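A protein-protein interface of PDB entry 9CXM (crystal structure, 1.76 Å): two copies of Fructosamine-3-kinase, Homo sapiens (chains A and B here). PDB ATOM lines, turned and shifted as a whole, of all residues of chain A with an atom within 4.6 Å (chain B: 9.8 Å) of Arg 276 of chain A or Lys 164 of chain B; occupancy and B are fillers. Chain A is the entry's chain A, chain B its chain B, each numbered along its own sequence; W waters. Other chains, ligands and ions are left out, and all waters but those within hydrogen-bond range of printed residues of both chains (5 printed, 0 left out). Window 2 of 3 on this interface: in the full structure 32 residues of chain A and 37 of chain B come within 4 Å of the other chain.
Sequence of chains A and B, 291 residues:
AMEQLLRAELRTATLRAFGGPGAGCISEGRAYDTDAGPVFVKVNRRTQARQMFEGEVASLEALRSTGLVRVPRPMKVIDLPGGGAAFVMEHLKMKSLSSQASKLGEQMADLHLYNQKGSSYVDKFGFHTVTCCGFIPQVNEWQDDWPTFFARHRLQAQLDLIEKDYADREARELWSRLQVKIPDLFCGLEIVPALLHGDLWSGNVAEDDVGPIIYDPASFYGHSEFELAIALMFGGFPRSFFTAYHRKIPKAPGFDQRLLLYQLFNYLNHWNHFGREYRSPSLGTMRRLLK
The side-chain carboxylate (OD1) of Asp 165 of chain B lies within salt-bridge range of the side-chain amino group (NZ) of Lys 164 of chain B, at 3.2 Å.
The side-chain hydroxyl (OH) of Tyr 166 of chain B is in hydrogen-bond range of the backbone carbonyl oxygen (O) of Trp 271 of chain B (2.9 Å).
Of the printed residues of chain B, Phe 274 of chain A touches Tyr 166 (3.5 Å) and Gly 275 (3.8 Å).
Gly 275 of chain A touches just these residues of chain B: Asp 165 and Tyr 166.
Of chain B, only Lys 164 and Asp 165 come within 4 Å of Arg 276 of chain A.
Lys 164 of chain B touches just one residue of chain A: Arg 276.
Printed residues of chain A within 4 Å of Asp 165 of chain B: Tyr 166, Gly 275 and Arg 276.
Of the printed residues of chain A, Tyr 166 of chain B touches Tyr 166 (3.6 Å), Phe 274 (3.5 Å) and Gly 275 (3.7 Å).
Of the printed residues of chain A, Gly 275 of chain B touches Phe 274.
Tyr 166 of chain A touches its own counterpart, Tyr 166 of chain B.
Gly 275 of chain A touches Tyr 166 of chain B, but with the chains exchanged Tyr 166 of chain A does not touch Gly 275 of chain B (8.7 Å).
Positions printed for both chains: 166, 271 and 275.
The backbone carbonyl oxygen (O) of Phe 274 of chain A is in hydrogen-bond range of the side-chain hydroxyl (OH) of Tyr 166 of chain B (3.5 Å).
The backbone NH of Arg 276 of chain A is in hydrogen-bond range of the backbone carbonyl oxygen of Asp 165 of chain B (2.9 Å).
Printed residues of chain B that touch a printed residue of chain A: Lys 164, Asp 165, Tyr 166 and Gly 275.
Hydrophobic or aromatic side chains of chain B that line the printed part of chain A: Tyr 166.
Among the printed residues, 8 pairs touch across the chains.
Among the printed residues, no Asp or Glu carboxylate lies within 4 Å of a Lys or Arg side-chain nitrogen of the other chain.
Among the printed residues, pairs that only touch across the chains: Gly 275 of chain A with Asp 165 of chain B, Arg 276 of chain A with Lys 164 of chain B, Tyr 166 of chain A with Asp 165 of chain B, Tyr 166 of chain A with Tyr 166 of chain B, Gly 275 of chain A with Tyr 166 of chain B and Phe 274 of chain A with Gly 275 of chain B.
Water W2 lies within hydrogen-bond range of OH of Tyr 166 of chain B (2.5 Å), O of Phe 274 of chain A (2.8 Å) and O of Asn 272 of chain B (3.0 Å).
Water W3 lies within hydrogen-bond range of O of Phe 274 of chain A (2.6 Å), N of Glu 277 of chain A (2.9 Å), N of Arg 276 of chain A (3.2 Å) and OD2 of Asp 165 of chain B (3.5 Å).
Water W1 lies within hydrogen-bond range of the side-chain carboxylate (OD1) of Asp 165 of chain B (2.7 Å) and the backbone NH (N) of Glu 277 of chain A (3.5 Å).
Water W4 lies within hydrogen-bond range of the backbone carbonyl oxygen of Lys 164 of chain B (2.9 Å) and the guanidinium group of Arg 276 of chain A (3.3 Å).
Water W5 lies within hydrogen-bond range of OE1 of Glu 277 of chain A (2.9 Å) and OD2 of Asp 165 of chain B (3.4 Å).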
ATOM      1  N   TYR A 166      -9.789  36.483   1.271  1.00  0.00           N
ATOM      2  CA  TYR A 166     -10.779  36.621   0.227  1.00  0.00           C
ATOM      3  C   TYR A 166     -11.092  38.059  -0.110  1.00  0.00           C
ATOM      4  O   TYR A 166     -11.644  38.294  -1.186  1.00  0.00           O
ATOM      5  CB  TYR A 166     -12.110  35.927   0.582  1.00  0.00           C
ATOM      6  CG  TYR A 166     -12.006  34.433   0.741  1.00  0.00           C
ATOM      7  CD1 TYR A 166     -12.147  33.574  -0.354  1.00  0.00           C
ATOM      8  CD2 TYR A 166     -11.706  33.886   1.959  1.00  0.00           C
ATOM      9  CE1 TYR A 166     -12.034  32.184  -0.197  1.00  0.00           C
ATOM     10  CE2 TYR A 166     -11.571  32.535   2.131  1.00  0.00           C
ATOM     11  CZ  TYR A 166     -11.719  31.683   1.042  1.00  0.00           C
ATOM     12  OH  TYR A 166     -11.595  30.335   1.244  1.00  0.00           O
ATOM     13  N   TRP A 271     -16.315  28.527   5.963  1.00  0.00           N
ATOM     14  CA  TRP A 271     -15.763  29.306   4.847  1.00  0.00           C
ATOM     15  C   TRP A 271     -14.239  29.343   4.923  1.00  0.00           C
ATOM     16  O   TRP A 271     -13.547  29.075   3.932  1.00  0.00           O
ATOM     17  CB  TRP A 271     -16.361  30.723   4.878  1.00  0.00           C
ATOM     18  CG  TRP A 271     -16.088  31.634   3.716  1.00  0.00           C
ATOM     19  CD1 TRP A 271     -15.225  31.413   2.645  1.00  0.00           C
ATOM     20  CD2 TRP A 271     -16.654  32.926   3.514  1.00  0.00           C
ATOM     21  NE1 TRP A 271     -15.248  32.512   1.787  1.00  0.00           N
ATOM     22  CE2 TRP A 271     -16.128  33.437   2.291  1.00  0.00           C
ATOM     23  CE3 TRP A 271     -17.583  33.714   4.238  1.00  0.00           C
ATOM     24  CZ2 TRP A 271     -16.467  34.689   1.812  1.00  0.00           C
ATOM     25  CZ3 TRP A 271     -17.912  34.965   3.746  1.00  0.00           C
ATOM     26  CH2 TRP A 271     -17.367  35.433   2.524  1.00  0.00           C
ATOM     27  N   PHE A 274     -13.038  25.497   4.213  1.00  0.00           N
ATOM     28  CA  PHE A 274     -13.426  24.780   3.003  1.00  0.00           C
ATOM     29  C   PHE A 274     -13.757  25.690   1.830  1.00  0.00           C
ATOM     30  O   PHE A 274     -14.082  25.197   0.741  1.00  0.00           O
ATOM     31  CB  PHE A 274     -14.630  23.876   3.330  1.00  0.00           C
ATOM     32  CG  PHE A 274     -14.419  23.027   4.548  1.00  0.00           C
ATOM     33  CD1 PHE A 274     -13.453  22.047   4.560  1.00  0.00           C
ATOM     34  CD2 PHE A 274     -15.201  23.164   5.667  1.00  0.00           C
ATOM     35  CE1 PHE A 274     -13.239  21.236   5.700  1.00  0.00           C
ATOM     36  CE2 PHE A 274     -15.010  22.377   6.786  1.00  0.00           C
ATOM     37  CZ  PHE A 274     -14.023  21.393   6.810  1.00  0.00           C
ATOM     38  N   GLY A 275     -13.727  26.997   2.015  1.00  0.00           N
ATOM     39  CA  GLY A 275     -13.902  27.887   0.915  1.00  0.00           C
ATOM     40  C   GLY A 275     -15.321  28.369   0.708  1.00  0.00           C
ATOM     41  O   GLY A 275     -16.214  28.323   1.572  1.00  0.00           O
ATOM     42  N   ARG A 276     -15.509  28.867  -0.503  1.00  0.00           N
ATOM     43  CA  ARG A 276     -16.643  29.686  -0.887  1.00  0.00           C
ATOM     44  C   ARG A 276     -17.970  28.954  -0.954  1.00  0.00           C
ATOM     45  O   ARG A 276     -18.998  29.633  -1.089  1.00  0.00           O
ATOM     46  CB  ARG A 276     -16.361  30.381  -2.223  1.00  0.00           C
ATOM     47  CG  ARG A 276     -15.691  31.743  -2.043  1.00  0.00           C
ATOM     48  CD  ARG A 276     -15.194  32.275  -3.412  1.00  0.00           C
ATOM     49  NE  ARG A 276     -15.716  33.628  -3.616  1.00  0.00           N
ATOM     50  CZ  ARG A 276     -16.782  33.936  -4.354  1.00  0.00           C
ATOM     51  NH1 ARG A 276     -17.451  33.016  -5.036  1.00  0.00           N
ATOM     52  NH2 ARG A 276     -17.204  35.196  -4.391  1.00  0.00           N
ATOM     53  N   GLU A 277     -17.997  27.629  -0.862  1.00  0.00           N
ATOM     54  CA  GLU A 277     -19.264  26.920  -0.672  1.00  0.00           C
ATOM     55  C   GLU A 277     -19.991  27.476   0.561  1.00  0.00           C
ATOM     56  O   GLU A 277     -21.224  27.473   0.614  1.00  0.00           O
ATOM     57  CB  GLU A 277     -19.037  25.425  -0.498  1.00  0.00           C
ATOM     58  CG  GLU A 277     -20.272  24.633  -0.082  1.00  0.00           C
ATOM     59  CD  GLU A 277     -19.955  23.178   0.260  1.00  0.00           C
ATOM     60  OE1 GLU A 277     -18.763  22.771   0.176  1.00  0.00           O
ATOM     61  OE2 GLU A 277     -20.890  22.445   0.665  1.00  0.00           O
ATOM     62  N   TYR A 278     -19.242  27.995   1.527  1.00  0.00           N
ATOM     63  CA  TYR A 278     -19.858  28.503   2.761  1.00  0.00           C
ATOM     64  C   TYR A 278     -20.029  30.013   2.764  1.00  0.00           C
ATOM     65  O   TYR A 278     -20.480  30.592   3.789  1.00  0.00           O
ATOM     66  CB  TYR A 278     -19.047  28.032   3.962  1.00  0.00           C
ATOM     67  CG  TYR A 278     -19.227  26.550   4.138  1.00  0.00           C
ATOM     68  CD1 TYR A 278     -20.374  26.014   4.792  1.00  0.00           C
ATOM     69  CD2 TYR A 278     -18.294  25.661   3.637  1.00  0.00           C
ATOM     70  CE1 TYR A 278     -20.545  24.675   4.944  1.00  0.00           C
ATOM     71  CE2 TYR A 278     -18.477  24.291   3.792  1.00  0.00           C
ATOM     72  CZ  TYR A 278     -19.605  23.815   4.435  1.00  0.00           C
ATOM     73  OH  TYR A 278     -19.785  22.465   4.598  1.00  0.00           O
ATOM     74  N   ARG A 279     -19.762  30.676   1.627  1.00  0.00           N
ATOM     75  CA  ARG A 279     -19.971  32.120   1.571  1.00  0.00           C
ATOM     76  C   ARG A 279     -21.453  32.456   1.635  1.00  0.00           C
ATOM     77  O   ARG A 279     -21.855  33.363   2.375  1.00  0.00           O
ATOM     78  CB  ARG A 279     -19.355  32.711   0.288  1.00  0.00           C
ATOM     79  CG  ARG A 279     -19.622  34.206   0.152  1.00  0.00           C
ATOM     80  CD  ARG A 279     -18.878  34.702  -1.174  1.00  0.00           C
ATOM     81  NE  ARG A 279     -18.995  36.143  -1.304  1.00  0.00           N
ATOM     82  CZ  ARG A 279     -20.021  36.730  -1.896  1.00  0.00           C
ATOM     83  NH1 ARG A 279     -21.021  36.016  -2.388  1.00  0.00           N
ATOM     84  NH2 ARG A 279     -20.060  38.063  -1.961  1.00  0.00           N
ATOM     85  N   SER A 280     -22.272  31.718   0.900  1.00  0.00           N
ATOM     86  CA  SER A 280     -23.696  32.027   0.847  1.00  0.00           C
ATOM     87  C   SER A 280     -24.360  31.881   2.215  1.00  0.00           C
ATOM     88  O   SER A 280     -25.056  32.821   2.633  1.00  0.00           O
ATOM     89  CB  SER A 280     -24.365  31.135  -0.196  1.00  0.00           C
ATOM     90  OG  SER A 280     -25.773  31.281  -0.171  1.00  0.00           O
ATOM     91  N   ILE B 136     -15.040  14.240  -6.605  1.00  0.00           N
ATOM     92  CA  ILE B 136     -14.779  15.174  -7.697  1.00  0.00           C
ATOM     93  C   ILE B 136     -14.762  14.409  -9.020  1.00  0.00           C
ATOM     94  O   ILE B 136     -13.886  13.546  -9.215  1.00  0.00           O
ATOM     95  CB  ILE B 136     -13.451  15.914  -7.477  1.00  0.00           C
ATOM     96  CG1 ILE B 136     -13.555  16.825  -6.273  1.00  0.00           C
ATOM     97  CG2 ILE B 136     -13.044  16.701  -8.709  1.00  0.00           C
ATOM     98  CD1 ILE B 136     -12.147  17.244  -5.715  1.00  0.00           C
ATOM     99  N   GLN B 156      -4.415  20.754 -13.533  1.00  0.00           N
ATOM    100  CA  GLN B 156      -5.182  21.977 -13.851  1.00  0.00           C
ATOM    101  C   GLN B 156      -6.622  21.870 -13.348  1.00  0.00           C
ATOM    102  O   GLN B 156      -7.193  22.834 -12.816  1.00  0.00           O
ATOM    103  CB  GLN B 156      -5.164  22.219 -15.382  1.00  0.00           C
ATOM    104  CG  GLN B 156      -6.004  23.527 -15.719  1.00  0.00           C
ATOM    105  CD  GLN B 156      -5.163  24.708 -15.542  1.00  0.00           C
ATOM    106  OE1 GLN B 156      -4.037  24.745 -16.034  1.00  0.00           O
ATOM    107  NE2 GLN B 156      -5.664  25.699 -14.741  1.00  0.00           N
ATOM    108  N   ALA B 157      -7.233  20.696 -13.473  1.00  0.00           N
ATOM    109  CA  ALA B 157      -8.571  20.507 -12.932  1.00  0.00           C
ATOM    110  C   ALA B 157      -8.627  20.806 -11.417  1.00  0.00           C
ATOM    111  O   ALA B 157      -9.514  21.531 -10.937  1.00  0.00           O
ATOM    112  CB  ALA B 157      -9.043  19.075 -13.233  1.00  0.00           C
ATOM    113  N   GLN B 158      -7.680  20.252 -10.646  1.00  0.00           N
ATOM    114  CA  GLN B 158      -7.671  20.519  -9.210  1.00  0.00           C
ATOM    115  C   GLN B 158      -7.433  21.999  -8.924  1.00  0.00           C
ATOM    116  O   GLN B 158      -8.038  22.597  -8.016  1.00  0.00           O
ATOM    117  CB  GLN B 158      -6.592  19.684  -8.553  1.00  0.00           C
ATOM    118  CG  GLN B 158      -6.964  18.153  -8.654  1.00  0.00           C
ATOM    119  CD  GLN B 158      -7.988  17.773  -7.600  1.00  0.00           C
ATOM    120  OE1 GLN B 158      -8.146  18.476  -6.609  1.00  0.00           O
ATOM    121  NE2 GLN B 158      -8.610  16.617  -7.758  1.00  0.00           N
ATOM    122  N   LEU B 159      -6.513  22.607  -9.671  1.00  0.00           N
ATOM    123  CA  LEU B 159      -6.179  24.028  -9.389  1.00  0.00           C
ATOM    124  C   LEU B 159      -7.273  24.981  -9.849  1.00  0.00           C
ATOM    125  O   LEU B 159      -7.455  26.038  -9.216  1.00  0.00           O
ATOM    126  CB  LEU B 159      -4.816  24.389 -10.016  1.00  0.00           C
ATOM    127  CG  LEU B 159      -3.678  23.756  -9.180  1.00  0.00           C
ATOM    128  CD1 LEU B 159      -2.396  23.378  -9.972  1.00  0.00           C
ATOM    129  CD2 LEU B 159      -3.359  24.736  -8.053  1.00  0.00           C
ATOM    130  N   ASP B 160      -8.056  24.617 -10.872  1.00  0.00           N
ATOM    131  CA  ASP B 160      -9.232  25.428 -11.205  1.00  0.00           C
ATOM    132  C   ASP B 160     -10.266  25.408 -10.071  1.00  0.00           C
ATOM    133  O   ASP B 160     -10.934  26.430  -9.789  1.00  0.00           O
ATOM    134  CB  ASP B 160      -9.863  24.924 -12.479  1.00  0.00           C
ATOM    135  CG  ASP B 160      -9.064  25.335 -13.731  1.00  0.00           C
ATOM    136  OD1 ASP B 160      -8.153  26.174 -13.633  1.00  0.00           O
ATOM    137  OD2 ASP B 160      -9.347  24.746 -14.778  1.00  0.00           O
ATOM    138  N   LEU B 161     -10.457  24.248  -9.454  1.00  0.00           N
ATOM    139  CA  LEU B 161     -11.343  24.169  -8.286  1.00  0.00           C
ATOM    140  C   LEU B 161     -10.777  24.939  -7.100  1.00  0.00           C
ATOM    141  O   LEU B 161     -11.517  25.616  -6.385  1.00  0.00           O
ATOM    142  CB  LEU B 161     -11.583  22.675  -7.954  1.00  0.00           C
ATOM    143  CG  LEU B 161     -12.646  22.330  -6.934  1.00  0.00           C
ATOM    144  CD1 LEU B 161     -13.943  23.070  -7.236  1.00  0.00           C
ATOM    145  CD2 LEU B 161     -12.839  20.803  -6.943  1.00  0.00           C
ATOM    146  N   ILE B 162      -9.468  24.866  -6.856  1.00  0.00           N
ATOM    147  CA  ILE B 162      -8.891  25.707  -5.813  1.00  0.00           C
ATOM    148  C   ILE B 162      -9.123  27.177  -6.095  1.00  0.00           C
ATOM    149  O   ILE B 162      -9.464  27.947  -5.181  1.00  0.00           O
ATOM    150  CB  ILE B 162      -7.404  25.392  -5.662  1.00  0.00           C
ATOM    151  CG1 ILE B 162      -7.328  24.092  -4.825  1.00  0.00           C
ATOM    152  CG2 ILE B 162      -6.643  26.480  -4.932  1.00  0.00           C
ATOM    153  CD1 ILE B 162      -6.172  23.320  -5.174  1.00  0.00           C
ATOM    154  N   GLU B 163      -8.972  27.593  -7.351  1.00  0.00           N
ATOM    155  CA  GLU B 163      -9.240  29.012  -7.675  1.00  0.00           C
ATOM    156  C   GLU B 163     -10.708  29.350  -7.456  1.00  0.00           C
ATOM    157  O   GLU B 163     -11.051  30.440  -6.943  1.00  0.00           O
ATOM    158  CB  GLU B 163      -8.842  29.302  -9.112  1.00  0.00           C
ATOM    159  CG  GLU B 163      -9.154  30.749  -9.617  1.00  0.00           C
ATOM    160  CD  GLU B 163      -8.470  31.821  -8.798  1.00  0.00           C
ATOM    161  OE1 GLU B 163      -7.387  31.633  -8.227  1.00  0.00           O
ATOM    162  OE2 GLU B 163      -9.002  32.928  -8.760  1.00  0.00           O
ATOM    163  N   LYS B 164     -11.604  28.473  -7.872  1.00  0.00           N
ATOM    164  CA  LYS B 164     -13.009  28.812  -7.671  1.00  0.00           C
ATOM    165  C   LYS B 164     -13.352  28.896  -6.176  1.00  0.00           C
ATOM    166  O   LYS B 164     -14.058  29.825  -5.731  1.00  0.00           O
ATOM    167  CB  LYS B 164     -13.895  27.801  -8.386  1.00  0.00           C
ATOM    168  CG  LYS B 164     -15.392  27.934  -8.017  1.00  0.00           C
ATOM    169  CD  LYS B 164     -16.282  27.012  -8.841  1.00  0.00           C
ATOM    170  CE  LYS B 164     -16.107  25.585  -8.384  1.00  0.00           C
ATOM    171  NZ  LYS B 164     -17.102  25.159  -7.326  1.00  0.00           N
ATOM    172  N   ASP B 165     -12.882  27.950  -5.376  1.00  0.00           N
ATOM    173  CA  ASP B 165     -13.362  27.910  -3.980  1.00  0.00           C
ATOM    174  C   ASP B 165     -12.507  28.695  -2.987  1.00  0.00           C
ATOM    175  O   ASP B 165     -13.019  29.176  -1.942  1.00  0.00           O
ATOM    176  CB  ASP B 165     -13.449  26.444  -3.531  1.00  0.00           C
ATOM    177  CG  ASP B 165     -14.560  25.696  -4.242  1.00  0.00           C
ATOM    178  OD1 ASP B 165     -15.393  26.339  -4.895  1.00  0.00           O
ATOM    179  OD2 ASP B 165     -14.624  24.453  -4.171  1.00  0.00           O
ATOM    180  N   TYR B 166     -11.220  28.847  -3.264  1.00  0.00           N
ATOM    181  CA  TYR B 166     -10.320  29.496  -2.343  1.00  0.00           C
ATOM    182  C   TYR B 166      -9.688  30.761  -2.896  1.00  0.00           C
ATOM    183  O   TYR B 166      -9.045  31.475  -2.120  1.00  0.00           O
ATOM    184  CB  TYR B 166      -9.211  28.543  -1.879  1.00  0.00           C
ATOM    185  CG  TYR B 166      -9.690  27.293  -1.197  1.00  0.00           C
ATOM    186  CD1 TYR B 166      -9.939  27.259   0.197  1.00  0.00           C
ATOM    187  CD2 TYR B 166      -9.844  26.124  -1.905  1.00  0.00           C
ATOM    188  CE1 TYR B 166     -10.381  26.047   0.825  1.00  0.00           C
ATOM    189  CE2 TYR B 166     -10.273  24.929  -1.282  1.00  0.00           C
ATOM    190  CZ  TYR B 166     -10.554  24.905   0.079  1.00  0.00           C
ATOM    191  OH  TYR B 166     -10.962  23.701   0.627  1.00  0.00           O
ATOM    192  N   ALA B 167      -9.757  30.986  -4.214  1.00  0.00           N
ATOM    193  CA  ALA B 167      -9.151  32.158  -4.882  1.00  0.00           C
ATOM    194  C   ALA B 167      -7.727  32.404  -4.378  1.00  0.00           C
ATOM    195  O   ALA B 167      -7.339  33.512  -3.991  1.00  0.00           O
ATOM    196  CB  ALA B 167     -10.037  33.390  -4.687  1.00  0.00           C
ATOM    197  N   ASP B 168      -6.933  31.342  -4.348  1.00  0.00           N
ATOM    198  CA  ASP B 168      -5.632  31.400  -3.707  1.00  0.00           C
ATOM    199  C   ASP B 168      -4.589  31.949  -4.676  1.00  0.00           C
ATOM    200  O   ASP B 168      -4.219  31.286  -5.648  1.00  0.00           O
ATOM    201  CB  ASP B 168      -5.254  30.016  -3.195  1.00  0.00           C
ATOM    202  CG  ASP B 168      -4.131  30.082  -2.226  1.00  0.00           C
ATOM    203  OD1 ASP B 168      -2.983  30.209  -2.682  1.00  0.00           O
ATOM    204  OD2 ASP B 168      -4.368  30.026  -0.986  1.00  0.00           O
ATOM    205  N   ARG B 169      -4.099  33.171  -4.411  1.00  0.00           N
ATOM    206  CA  ARG B 169      -3.149  33.781  -5.327  1.00  0.00           C
ATOM    207  C   ARG B 169      -1.873  32.984  -5.444  1.00  0.00           C
ATOM    208  O   ARG B 169      -1.368  32.782  -6.569  1.00  0.00           O
ATOM    209  CB  ARG B 169      -2.788  35.204  -4.865  1.00  0.00           C
ATOM    210  CG  ARG B 169      -2.003  35.911  -5.962  1.00  0.00           C
ATOM    211  CD  ARG B 169      -1.077  36.952  -5.361  1.00  0.00           C
ATOM    212  NE  ARG B 169      -1.880  38.042  -4.820  1.00  0.00           N
ATOM    213  CZ  ARG B 169      -2.580  38.911  -5.542  1.00  0.00           C
ATOM    214  NH1 ARG B 169      -2.567  38.883  -6.872  1.00  0.00           N
ATOM    215  NH2 ARG B 169      -3.315  39.828  -4.914  1.00  0.00           N
ATOM    216  N   ALA B 171      -1.250  29.756  -5.017  1.00  0.00           N
ATOM    217  CA  ALA B 171      -1.415  28.539  -5.827  1.00  0.00           C
ATOM    218  C   ALA B 171      -1.449  28.864  -7.313  1.00  0.00           C
ATOM    219  O   ALA B 171      -0.799  28.181  -8.120  1.00  0.00           O
ATOM    220  CB  ALA B 171      -2.703  27.804  -5.403  1.00  0.00           C
ATOM    221  N   ARG B 172      -2.136  29.954  -7.689  1.00  0.00           N
ATOM    222  CA  ARG B 172      -2.247  30.369  -9.081  1.00  0.00           C
ATOM    223  C   ARG B 172      -0.880  30.693  -9.668  1.00  0.00           C
ATOM    224  O   ARG B 172      -0.534  30.241 -10.778  1.00  0.00           O
ATOM    225  CB  ARG B 172      -3.163  31.605  -9.147  1.00  0.00           C
ATOM    226  CG  ARG B 172      -3.958  31.804 -10.367  1.00  0.00           C
ATOM    227  CD  ARG B 172      -5.074  32.879 -10.102  1.00  0.00           C
ATOM    228  NE  ARG B 172      -4.544  34.076  -9.469  1.00  0.00           N
ATOM    229  CZ  ARG B 172      -5.025  34.619  -8.356  1.00  0.00           C
ATOM    230  NH1 ARG B 172      -6.060  34.084  -7.707  1.00  0.00           N
ATOM    231  NH2 ARG B 172      -4.454  35.719  -7.873  1.00  0.00           N
ATOM    232  N   TRP B 271      -6.734  19.083  -0.427  1.00  0.00           N
ATOM    233  CA  TRP B 271      -7.161  20.462  -0.179  1.00  0.00           C
ATOM    234  C   TRP B 271      -8.600  20.666  -0.634  1.00  0.00           C
ATOM    235  O   TRP B 271      -9.430  21.243   0.102  1.00  0.00           O
ATOM    236  CB  TRP B 271      -6.177  21.414  -0.895  1.00  0.00           C
ATOM    237  CG  TRP B 271      -6.313  22.918  -0.608  1.00  0.00           C
ATOM    238  CD1 TRP B 271      -7.285  23.563   0.167  1.00  0.00           C
ATOM    239  CD2 TRP B 271      -5.454  23.937  -1.114  1.00  0.00           C
ATOM    240  NE1 TRP B 271      -7.058  24.948   0.140  1.00  0.00           N
ATOM    241  CE2 TRP B 271      -5.949  25.198  -0.645  1.00  0.00           C
ATOM    242  CE3 TRP B 271      -4.317  23.921  -1.946  1.00  0.00           C
ATOM    243  CZ2 TRP B 271      -5.337  26.425  -1.011  1.00  0.00           C
ATOM    244  CZ3 TRP B 271      -3.708  25.115  -2.290  1.00  0.00           C
ATOM    245  CH2 TRP B 271      -4.205  26.377  -1.803  1.00  0.00           C
ATOM    246  N   ASN B 272      -8.934  20.201  -1.833  1.00  0.00           N
ATOM    247  CA  ASN B 272     -10.300  20.342  -2.311  1.00  0.00           C
ATOM    248  C   ASN B 272     -11.294  19.508  -1.499  1.00  0.00           C
ATOM    249  O   ASN B 272     -12.390  19.987  -1.201  1.00  0.00           O
ATOM    250  CB  ASN B 272     -10.403  19.984  -3.784  1.00  0.00           C
ATOM    251  CG  ASN B 272      -9.999  21.165  -4.667  1.00  0.00           C
ATOM    252  OD1 ASN B 272     -10.392  22.329  -4.383  1.00  0.00           O
ATOM    253  ND2 ASN B 272      -9.191  20.893  -5.729  1.00  0.00           N
ATOM    254  N   GLY B 275     -10.037  20.642   2.897  1.00  0.00           N
ATOM    255  CA  GLY B 275      -9.835  22.057   3.272  1.00  0.00           C
ATOM    256  C   GLY B 275      -8.404  22.494   3.484  1.00  0.00           C
ATOM    257  O   GLY B 275      -7.432  21.816   3.150  1.00  0.00           O
HETATM  258  O   HOH W   1     -17.483  28.009  -4.290  1.00  0.00           O
HETATM  259  O   HOH W   2     -13.143  22.688  -0.122  1.00  0.00           O
HETATM  260  O   HOH W   3     -15.764  25.723  -1.135  1.00  0.00           O
HETATM  261  O   HOH W   4     -15.787  31.430  -7.346  1.00  0.00           O
HETATM  262  O   HOH W   5     -16.673  23.170  -1.765  1.00  0.00           O
